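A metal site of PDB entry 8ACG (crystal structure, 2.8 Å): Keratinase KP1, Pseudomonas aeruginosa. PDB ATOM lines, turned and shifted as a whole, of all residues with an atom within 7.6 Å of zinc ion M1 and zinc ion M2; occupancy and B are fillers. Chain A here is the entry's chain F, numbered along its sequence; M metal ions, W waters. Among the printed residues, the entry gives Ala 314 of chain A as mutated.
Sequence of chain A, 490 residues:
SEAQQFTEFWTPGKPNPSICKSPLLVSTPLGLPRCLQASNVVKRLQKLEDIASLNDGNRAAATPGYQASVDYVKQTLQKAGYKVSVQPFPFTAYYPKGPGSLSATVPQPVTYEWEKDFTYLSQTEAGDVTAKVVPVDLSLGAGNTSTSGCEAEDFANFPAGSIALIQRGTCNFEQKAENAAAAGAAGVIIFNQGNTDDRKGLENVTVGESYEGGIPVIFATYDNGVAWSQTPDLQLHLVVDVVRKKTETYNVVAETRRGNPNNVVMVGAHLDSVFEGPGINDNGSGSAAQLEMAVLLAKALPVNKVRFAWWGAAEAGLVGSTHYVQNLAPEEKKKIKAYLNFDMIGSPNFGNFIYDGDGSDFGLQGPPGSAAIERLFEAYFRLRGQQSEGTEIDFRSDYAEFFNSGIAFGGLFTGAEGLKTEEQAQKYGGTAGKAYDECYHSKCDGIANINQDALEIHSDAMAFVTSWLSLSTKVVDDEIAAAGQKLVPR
The side-chain carboxylate (OD2) of Asp 343 is in hydrogen-bond range of the side-chain hydroxyl (OG) of Ser 397, 2.7 Å away. The side-chain hydroxyl (OH) of Tyr 440 lies close to a ring nitrogen (NE2) of His 441, at 3.4 Å. The side-chain carboxylate of Asp 272 lies within hydrogen-bond range of the backbone NH of Glu 315, 3.0 Å away. The backbone carbonyl oxygen (O) of His 270 lies within hydrogen-bond range of the side-chain amide nitrogen (ND2) of Asn 283 (3.2 Å). The backbone carbonyl oxygen (O) of Asp 272 sits at hydrogen-bond distance from a ring nitrogen (ND1) of His 270 (3.0 Å).
OH of Tyr 440 touches zinc ion M1, at 3.9 Å. The nearest printed residue that does not touch zinc ion M1 is His 270 (4.6 Å).
Of the 22 residues printed, 4 come within 4 Å of zinc ion M2.
Zinc ion M1 is bound by NE2 of His 441 (2.2 Å). OD2 of Asp 282 is bound to zinc ion M1 (2.3 Å). Zinc ion M1 is bound by OE2 of Glu 315 (2.3 Å). Slightly farther from zinc ion M1 lies the side-chain carboxylate (OE1) of Glu 315 (2.6 Å).
Zinc ion M2 is bound by OD1 of Asp 343. Zinc ion M2 is bound by OD1 of Asp 282. Zinc ion M2 is bound by NE2 of His 270, 2.5 Å away. Slightly farther from zinc ion M2 lies OD2 of Asp 343 (2.6 Å).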
ATOM      1  N   HIS A 270       1.095 -22.164 -20.846  1.00  0.00           N
ATOM      2  CA  HIS A 270       0.836 -23.275 -19.937  1.00  0.00           C
ATOM      3  C   HIS A 270      -0.480 -23.915 -20.325  1.00  0.00           C
ATOM      4  O   HIS A 270      -1.449 -23.214 -20.654  1.00  0.00           O
ATOM      5  CB  HIS A 270       0.822 -22.835 -18.462  1.00  0.00           C
ATOM      6  CG  HIS A 270      -0.411 -22.104 -18.007  1.00  0.00           C
ATOM      7  ND1 HIS A 270      -1.526 -22.748 -17.514  1.00  0.00           N
ATOM      8  CD2 HIS A 270      -0.677 -20.775 -17.914  1.00  0.00           C
ATOM      9  CE1 HIS A 270      -2.435 -21.862 -17.172  1.00  0.00           C
ATOM     10  NE2 HIS A 270      -1.943 -20.652 -17.398  1.00  0.00           N
ATOM     11  N   ASP A 272      -2.262 -26.500 -18.594  1.00  0.00           N
ATOM     12  CA  ASP A 272      -3.200 -26.951 -17.573  1.00  0.00           C
ATOM     13  C   ASP A 272      -4.138 -25.825 -17.137  1.00  0.00           C
ATOM     14  O   ASP A 272      -3.848 -24.636 -17.322  1.00  0.00           O
ATOM     15  CB  ASP A 272      -2.483 -27.463 -16.350  1.00  0.00           C
ATOM     16  CG  ASP A 272      -1.715 -26.362 -15.647  1.00  0.00           C
ATOM     17  OD1 ASP A 272      -0.989 -25.651 -16.375  1.00  0.00           O
ATOM     18  OD2 ASP A 272      -1.905 -26.183 -14.413  1.00  0.00           O
ATOM     19  N   SER A 273      -5.237 -26.221 -16.514  1.00  0.00           N
ATOM     20  CA  SER A 273      -6.202 -25.318 -15.916  1.00  0.00           C
ATOM     21  C   SER A 273      -6.273 -25.543 -14.403  1.00  0.00           C
ATOM     22  O   SER A 273      -5.682 -26.480 -13.857  1.00  0.00           O
ATOM     23  CB  SER A 273      -7.594 -25.521 -16.513  1.00  0.00           C
ATOM     24  OG  SER A 273      -8.188 -26.730 -16.024  1.00  0.00           O
ATOM     25  N   VAL A 274      -7.023 -24.670 -13.730  1.00  0.00           N
ATOM     26  CA  VAL A 274      -7.367 -24.899 -12.336  1.00  0.00           C
ATOM     27  C   VAL A 274      -8.340 -26.065 -12.303  1.00  0.00           C
ATOM     28  O   VAL A 274      -8.824 -26.505 -13.351  1.00  0.00           O
ATOM     29  CB  VAL A 274      -7.977 -23.660 -11.644  1.00  0.00           C
ATOM     30  CG1 VAL A 274      -7.025 -22.508 -11.632  1.00  0.00           C
ATOM     31  CG2 VAL A 274      -9.302 -23.295 -12.305  1.00  0.00           C
ATOM     32  N   ASN A 281      -9.793 -19.557 -21.355  1.00  0.00           N
ATOM     33  CA  ASN A 281      -8.996 -18.337 -21.439  1.00  0.00           C
ATOM     34  C   ASN A 281      -7.698 -18.493 -20.673  1.00  0.00           C
ATOM     35  O   ASN A 281      -6.637 -18.040 -21.117  1.00  0.00           O
ATOM     36  CB  ASN A 281      -9.805 -17.164 -20.884  1.00  0.00           C
ATOM     37  CG  ASN A 281      -9.099 -15.855 -21.008  1.00  0.00           C
ATOM     38  OD1 ASN A 281      -8.418 -15.595 -21.982  1.00  0.00           O
ATOM     39  ND2 ASN A 281      -9.291 -14.993 -20.045  1.00  0.00           N
ATOM     40  N   ASP A 282      -7.751 -19.112 -19.491  1.00  0.00           N
ATOM     41  CA  ASP A 282      -6.577 -19.319 -18.665  1.00  0.00           C
ATOM     42  C   ASP A 282      -6.321 -20.816 -18.571  1.00  0.00           C
ATOM     43  O   ASP A 282      -6.894 -21.483 -17.707  1.00  0.00           O
ATOM     44  CB  ASP A 282      -6.764 -18.701 -17.294  1.00  0.00           C
ATOM     45  CG  ASP A 282      -5.559 -18.853 -16.417  1.00  0.00           C
ATOM     46  OD1 ASP A 282      -4.445 -18.953 -16.970  1.00  0.00           O
ATOM     47  OD2 ASP A 282      -5.729 -18.909 -15.181  1.00  0.00           O
ATOM     48  N   ASN A 283      -5.472 -21.353 -19.444  1.00  0.00           N
ATOM     49  CA  ASN A 283      -4.777 -20.629 -20.512  1.00  0.00           C
ATOM     50  C   ASN A 283      -4.983 -21.380 -21.820  1.00  0.00           C
ATOM     51  O   ASN A 283      -4.032 -21.659 -22.534  1.00  0.00           O
ATOM     52  CB  ASN A 283      -3.278 -20.515 -20.223  1.00  0.00           C
ATOM     53  CG  ASN A 283      -2.530 -19.717 -21.264  1.00  0.00           C
ATOM     54  OD1 ASN A 283      -3.028 -18.747 -21.823  1.00  0.00           O
ATOM     55  ND2 ASN A 283      -1.324 -20.158 -21.563  1.00  0.00           N
ATOM     56  N   GLY A 284      -6.231 -21.749 -22.113  1.00  0.00           N
ATOM     57  CA  GLY A 284      -6.495 -22.308 -23.421  1.00  0.00           C
ATOM     58  C   GLY A 284      -6.148 -21.340 -24.525  1.00  0.00           C
ATOM     59  O   GLY A 284      -5.680 -21.749 -25.579  1.00  0.00           O
ATOM     60  N   ALA A 314       1.071 -25.533 -14.215  1.00  0.00           N
ATOM     61  CA  ALA A 314       1.456 -24.147 -13.921  1.00  0.00           C
ATOM     62  C   ALA A 314       0.591 -23.593 -12.812  1.00  0.00           C
ATOM     63  O   ALA A 314       1.086 -22.820 -11.986  1.00  0.00           O
ATOM     64  CB  ALA A 314       1.385 -23.260 -15.155  1.00  0.00           C
ATOM     65  N   GLU A 315      -0.695 -23.972 -12.790  1.00  0.00           N
ATOM     66  CA  GLU A 315      -1.566 -23.455 -11.741  1.00  0.00           C
ATOM     67  C   GLU A 315      -1.190 -23.975 -10.380  1.00  0.00           C
ATOM     68  O   GLU A 315      -1.789 -23.554  -9.389  1.00  0.00           O
ATOM     69  CB  GLU A 315      -3.047 -23.773 -12.039  1.00  0.00           C
ATOM     70  CG  GLU A 315      -3.524 -23.200 -13.377  1.00  0.00           C
ATOM     71  CD  GLU A 315      -3.689 -21.650 -13.374  1.00  0.00           C
ATOM     72  OE1 GLU A 315      -3.249 -21.000 -12.413  1.00  0.00           O
ATOM     73  OE2 GLU A 315      -4.178 -21.049 -14.347  1.00  0.00           O
ATOM     74  N   LEU A 318       3.937 -22.893 -11.153  1.00  0.00           N
ATOM     75  CA  LEU A 318       4.936 -22.874 -12.221  1.00  0.00           C
ATOM     76  C   LEU A 318       5.847 -24.104 -12.194  1.00  0.00           C
ATOM     77  O   LEU A 318       7.054 -24.017 -12.448  1.00  0.00           O
ATOM     78  CB  LEU A 318       5.762 -21.585 -12.152  1.00  0.00           C
ATOM     79  CG  LEU A 318       5.025 -20.267 -11.934  1.00  0.00           C
ATOM     80  CD1 LEU A 318       5.971 -19.099 -11.848  1.00  0.00           C
ATOM     81  CD2 LEU A 318       4.011 -20.031 -12.988  1.00  0.00           C
ATOM     82  N   ASN A 341       6.124 -15.531 -23.524  1.00  0.00           N
ATOM     83  CA  ASN A 341       5.152 -16.198 -22.683  1.00  0.00           C
ATOM     84  C   ASN A 341       3.794 -15.651 -23.046  1.00  0.00           C
ATOM     85  O   ASN A 341       3.636 -14.425 -23.128  1.00  0.00           O
ATOM     86  CB  ASN A 341       5.441 -15.969 -21.189  1.00  0.00           C
ATOM     87  CG  ASN A 341       4.652 -16.892 -20.298  1.00  0.00           C
ATOM     88  OD1 ASN A 341       4.906 -18.094 -20.311  1.00  0.00           O
ATOM     89  ND2 ASN A 341       3.718 -16.362 -19.518  1.00  0.00           N
ATOM     90  N   PHE A 342       2.821 -16.538 -23.295  1.00  0.00           N
ATOM     91  CA  PHE A 342       1.482 -16.122 -23.697  1.00  0.00           C
ATOM     92  C   PHE A 342       0.469 -16.804 -22.800  1.00  0.00           C
ATOM     93  O   PHE A 342       0.160 -17.974 -23.006  1.00  0.00           O
ATOM     94  CB  PHE A 342       1.214 -16.401 -25.163  1.00  0.00           C
ATOM     95  CG  PHE A 342       2.234 -15.769 -26.059  1.00  0.00           C
ATOM     96  CD1 PHE A 342       2.199 -14.409 -26.300  1.00  0.00           C
ATOM     97  CD2 PHE A 342       3.245 -16.519 -26.629  1.00  0.00           C
ATOM     98  CE1 PHE A 342       3.127 -13.828 -27.069  1.00  0.00           C
ATOM     99  CE2 PHE A 342       4.184 -15.917 -27.412  1.00  0.00           C
ATOM    100  CZ  PHE A 342       4.113 -14.565 -27.626  1.00  0.00           C
ATOM    101  N   ASP A 343      -0.020 -16.054 -21.802  1.00  0.00           N
ATOM    102  CA  ASP A 343      -0.852 -16.570 -20.719  1.00  0.00           C
ATOM    103  C   ASP A 343      -2.064 -15.651 -20.552  1.00  0.00           C
ATOM    104  O   ASP A 343      -1.928 -14.553 -20.012  1.00  0.00           O
ATOM    105  CB  ASP A 343      -0.053 -16.621 -19.429  1.00  0.00           C
ATOM    106  CG  ASP A 343      -0.756 -17.333 -18.309  1.00  0.00           C
ATOM    107  OD1 ASP A 343      -2.001 -17.451 -18.325  1.00  0.00           O
ATOM    108  OD2 ASP A 343      -0.056 -17.789 -17.381  1.00  0.00           O
ATOM    109  N   MET A 344      -3.245 -16.137 -20.962  1.00  0.00           N
ATOM    110  CA  MET A 344      -4.501 -15.391 -20.934  1.00  0.00           C
ATOM    111  C   MET A 344      -4.521 -14.253 -21.935  1.00  0.00           C
ATOM    112  O   MET A 344      -4.189 -13.120 -21.585  1.00  0.00           O
ATOM    113  CB  MET A 344      -4.799 -14.819 -19.555  1.00  0.00           C
ATOM    114  CG  MET A 344      -5.283 -15.807 -18.565  1.00  0.00           C
ATOM    115  SD  MET A 344      -5.612 -15.012 -16.993  1.00  0.00           S
ATOM    116  CE  MET A 344      -7.175 -14.207 -17.323  1.00  0.00           C
ATOM    117  N   ARG A 396       4.967 -14.015 -12.089  1.00  0.00           N
ATOM    118  CA  ARG A 396       3.580 -14.418 -11.935  1.00  0.00           C
ATOM    119  C   ARG A 396       3.177 -15.556 -12.879  1.00  0.00           C
ATOM    120  O   ARG A 396       2.099 -16.155 -12.692  1.00  0.00           O
ATOM    121  CB  ARG A 396       2.703 -13.209 -12.231  1.00  0.00           C
ATOM    122  CG  ARG A 396       3.086 -11.908 -11.548  1.00  0.00           C
ATOM    123  CD  ARG A 396       2.080 -10.792 -12.004  1.00  0.00           C
ATOM    124  NE  ARG A 396       2.265  -9.471 -11.385  1.00  0.00           N
ATOM    125  CZ  ARG A 396       1.532  -9.018 -10.360  1.00  0.00           C
ATOM    126  NH1 ARG A 396       1.751  -7.800  -9.837  1.00  0.00           N
ATOM    127  NH2 ARG A 396       0.596  -9.785  -9.817  1.00  0.00           N
ATOM    128  N   SER A 397       4.011 -15.859 -13.879  1.00  0.00           N
ATOM    129  CA  SER A 397       3.673 -16.850 -14.899  1.00  0.00           C
ATOM    130  C   SER A 397       4.966 -17.571 -15.292  1.00  0.00           C
ATOM    131  O   SER A 397       6.009 -17.373 -14.684  1.00  0.00           O
ATOM    132  CB  SER A 397       3.010 -16.145 -16.083  1.00  0.00           C
ATOM    133  OG  SER A 397       2.533 -17.093 -17.002  1.00  0.00           O
ATOM    134  N   ASP A 398       4.890 -18.404 -16.335  1.00  0.00           N
ATOM    135  CA  ASP A 398       5.926 -19.390 -16.637  1.00  0.00           C
ATOM    136  C   ASP A 398       7.221 -18.821 -17.176  1.00  0.00           C
ATOM    137  O   ASP A 398       8.114 -19.604 -17.447  1.00  0.00           O
ATOM    138  CB  ASP A 398       5.409 -20.432 -17.616  1.00  0.00           C
ATOM    139  CG  ASP A 398       4.294 -21.226 -17.038  1.00  0.00           C
ATOM    140  OD1 ASP A 398       4.578 -22.059 -16.131  1.00  0.00           O
ATOM    141  OD2 ASP A 398       3.134 -21.007 -17.432  1.00  0.00           O
ATOM    142  N   PHE A 413      -0.668 -10.284 -22.197  1.00  0.00           N
ATOM    143  CA  PHE A 413      -1.620 -10.493 -21.120  1.00  0.00           C
ATOM    144  C   PHE A 413      -2.810  -9.623 -21.451  1.00  0.00           C
ATOM    145  O   PHE A 413      -2.626  -8.497 -21.942  1.00  0.00           O
ATOM    146  CB  PHE A 413      -1.038 -10.090 -19.768  1.00  0.00           C
ATOM    147  CG  PHE A 413      -1.926 -10.406 -18.590  1.00  0.00           C
ATOM    148  CD1 PHE A 413      -2.603 -11.607 -18.518  1.00  0.00           C
ATOM    149  CD2 PHE A 413      -2.024  -9.529 -17.526  1.00  0.00           C
ATOM    150  CE1 PHE A 413      -3.400 -11.911 -17.413  1.00  0.00           C
ATOM    151  CE2 PHE A 413      -2.788  -9.837 -16.427  1.00  0.00           C
ATOM    152  CZ  PHE A 413      -3.481 -11.026 -16.365  1.00  0.00           C
ATOM    153  N   ALA A 416      -6.676 -10.145 -15.701  1.00  0.00           N
ATOM    154  CA  ALA A 416      -7.367 -11.187 -14.948  1.00  0.00           C
ATOM    155  C   ALA A 416      -8.323 -10.620 -13.922  1.00  0.00           C
ATOM    156  O   ALA A 416      -9.410 -10.171 -14.278  1.00  0.00           O
ATOM    157  CB  ALA A 416      -6.378 -12.139 -14.278  1.00  0.00           C
ATOM    158  N   TYR A 440     -12.405 -15.594 -14.168  1.00  0.00           N
ATOM    159  CA  TYR A 440     -11.040 -16.026 -13.852  1.00  0.00           C
ATOM    160  C   TYR A 440     -11.011 -17.145 -12.814  1.00  0.00           C
ATOM    161  O   TYR A 440     -11.592 -17.041 -11.735  1.00  0.00           O
ATOM    162  CB  TYR A 440     -10.263 -14.816 -13.342  1.00  0.00           C
ATOM    163  CG  TYR A 440      -8.888 -15.110 -12.827  1.00  0.00           C
ATOM    164  CD1 TYR A 440      -7.901 -15.623 -13.650  1.00  0.00           C
ATOM    165  CD2 TYR A 440      -8.570 -14.820 -11.512  1.00  0.00           C
ATOM    166  CE1 TYR A 440      -6.635 -15.865 -13.175  1.00  0.00           C
ATOM    167  CE2 TYR A 440      -7.316 -15.053 -11.020  1.00  0.00           C
ATOM    168  CZ  TYR A 440      -6.343 -15.587 -11.843  1.00  0.00           C
ATOM    169  OH  TYR A 440      -5.076 -15.824 -11.346  1.00  0.00           O
ATOM    170  N   HIS A 441     -10.338 -18.225 -13.192  1.00  0.00           N
ATOM    171  CA  HIS A 441     -10.167 -19.400 -12.357  1.00  0.00           C
ATOM    172  C   HIS A 441     -11.506 -19.981 -11.927  1.00  0.00           C
ATOM    173  O   HIS A 441     -11.591 -20.667 -10.913  1.00  0.00           O
ATOM    174  CB  HIS A 441      -9.283 -19.123 -11.151  1.00  0.00           C
ATOM    175  CG  HIS A 441      -7.839 -19.017 -11.502  1.00  0.00           C
ATOM    176  ND1 HIS A 441      -6.850 -18.806 -10.559  1.00  0.00           N
ATOM    177  CD2 HIS A 441      -7.209 -19.093 -12.696  1.00  0.00           C
ATOM    178  CE1 HIS A 441      -5.671 -18.779 -11.160  1.00  0.00           C
ATOM    179  NE2 HIS A 441      -5.860 -18.939 -12.456  1.00  0.00           N
HETATM  180 ZN    ZN M   1      -4.032 -18.839 -13.669  1.00  0.00          ZN
HETATM  181 ZN    ZN M   2      -2.464 -18.381 -16.511  1.00  0.00          ZN
HETATM  182  O   HOH W   1      -3.274 -16.039 -14.534  1.00  0.00           O
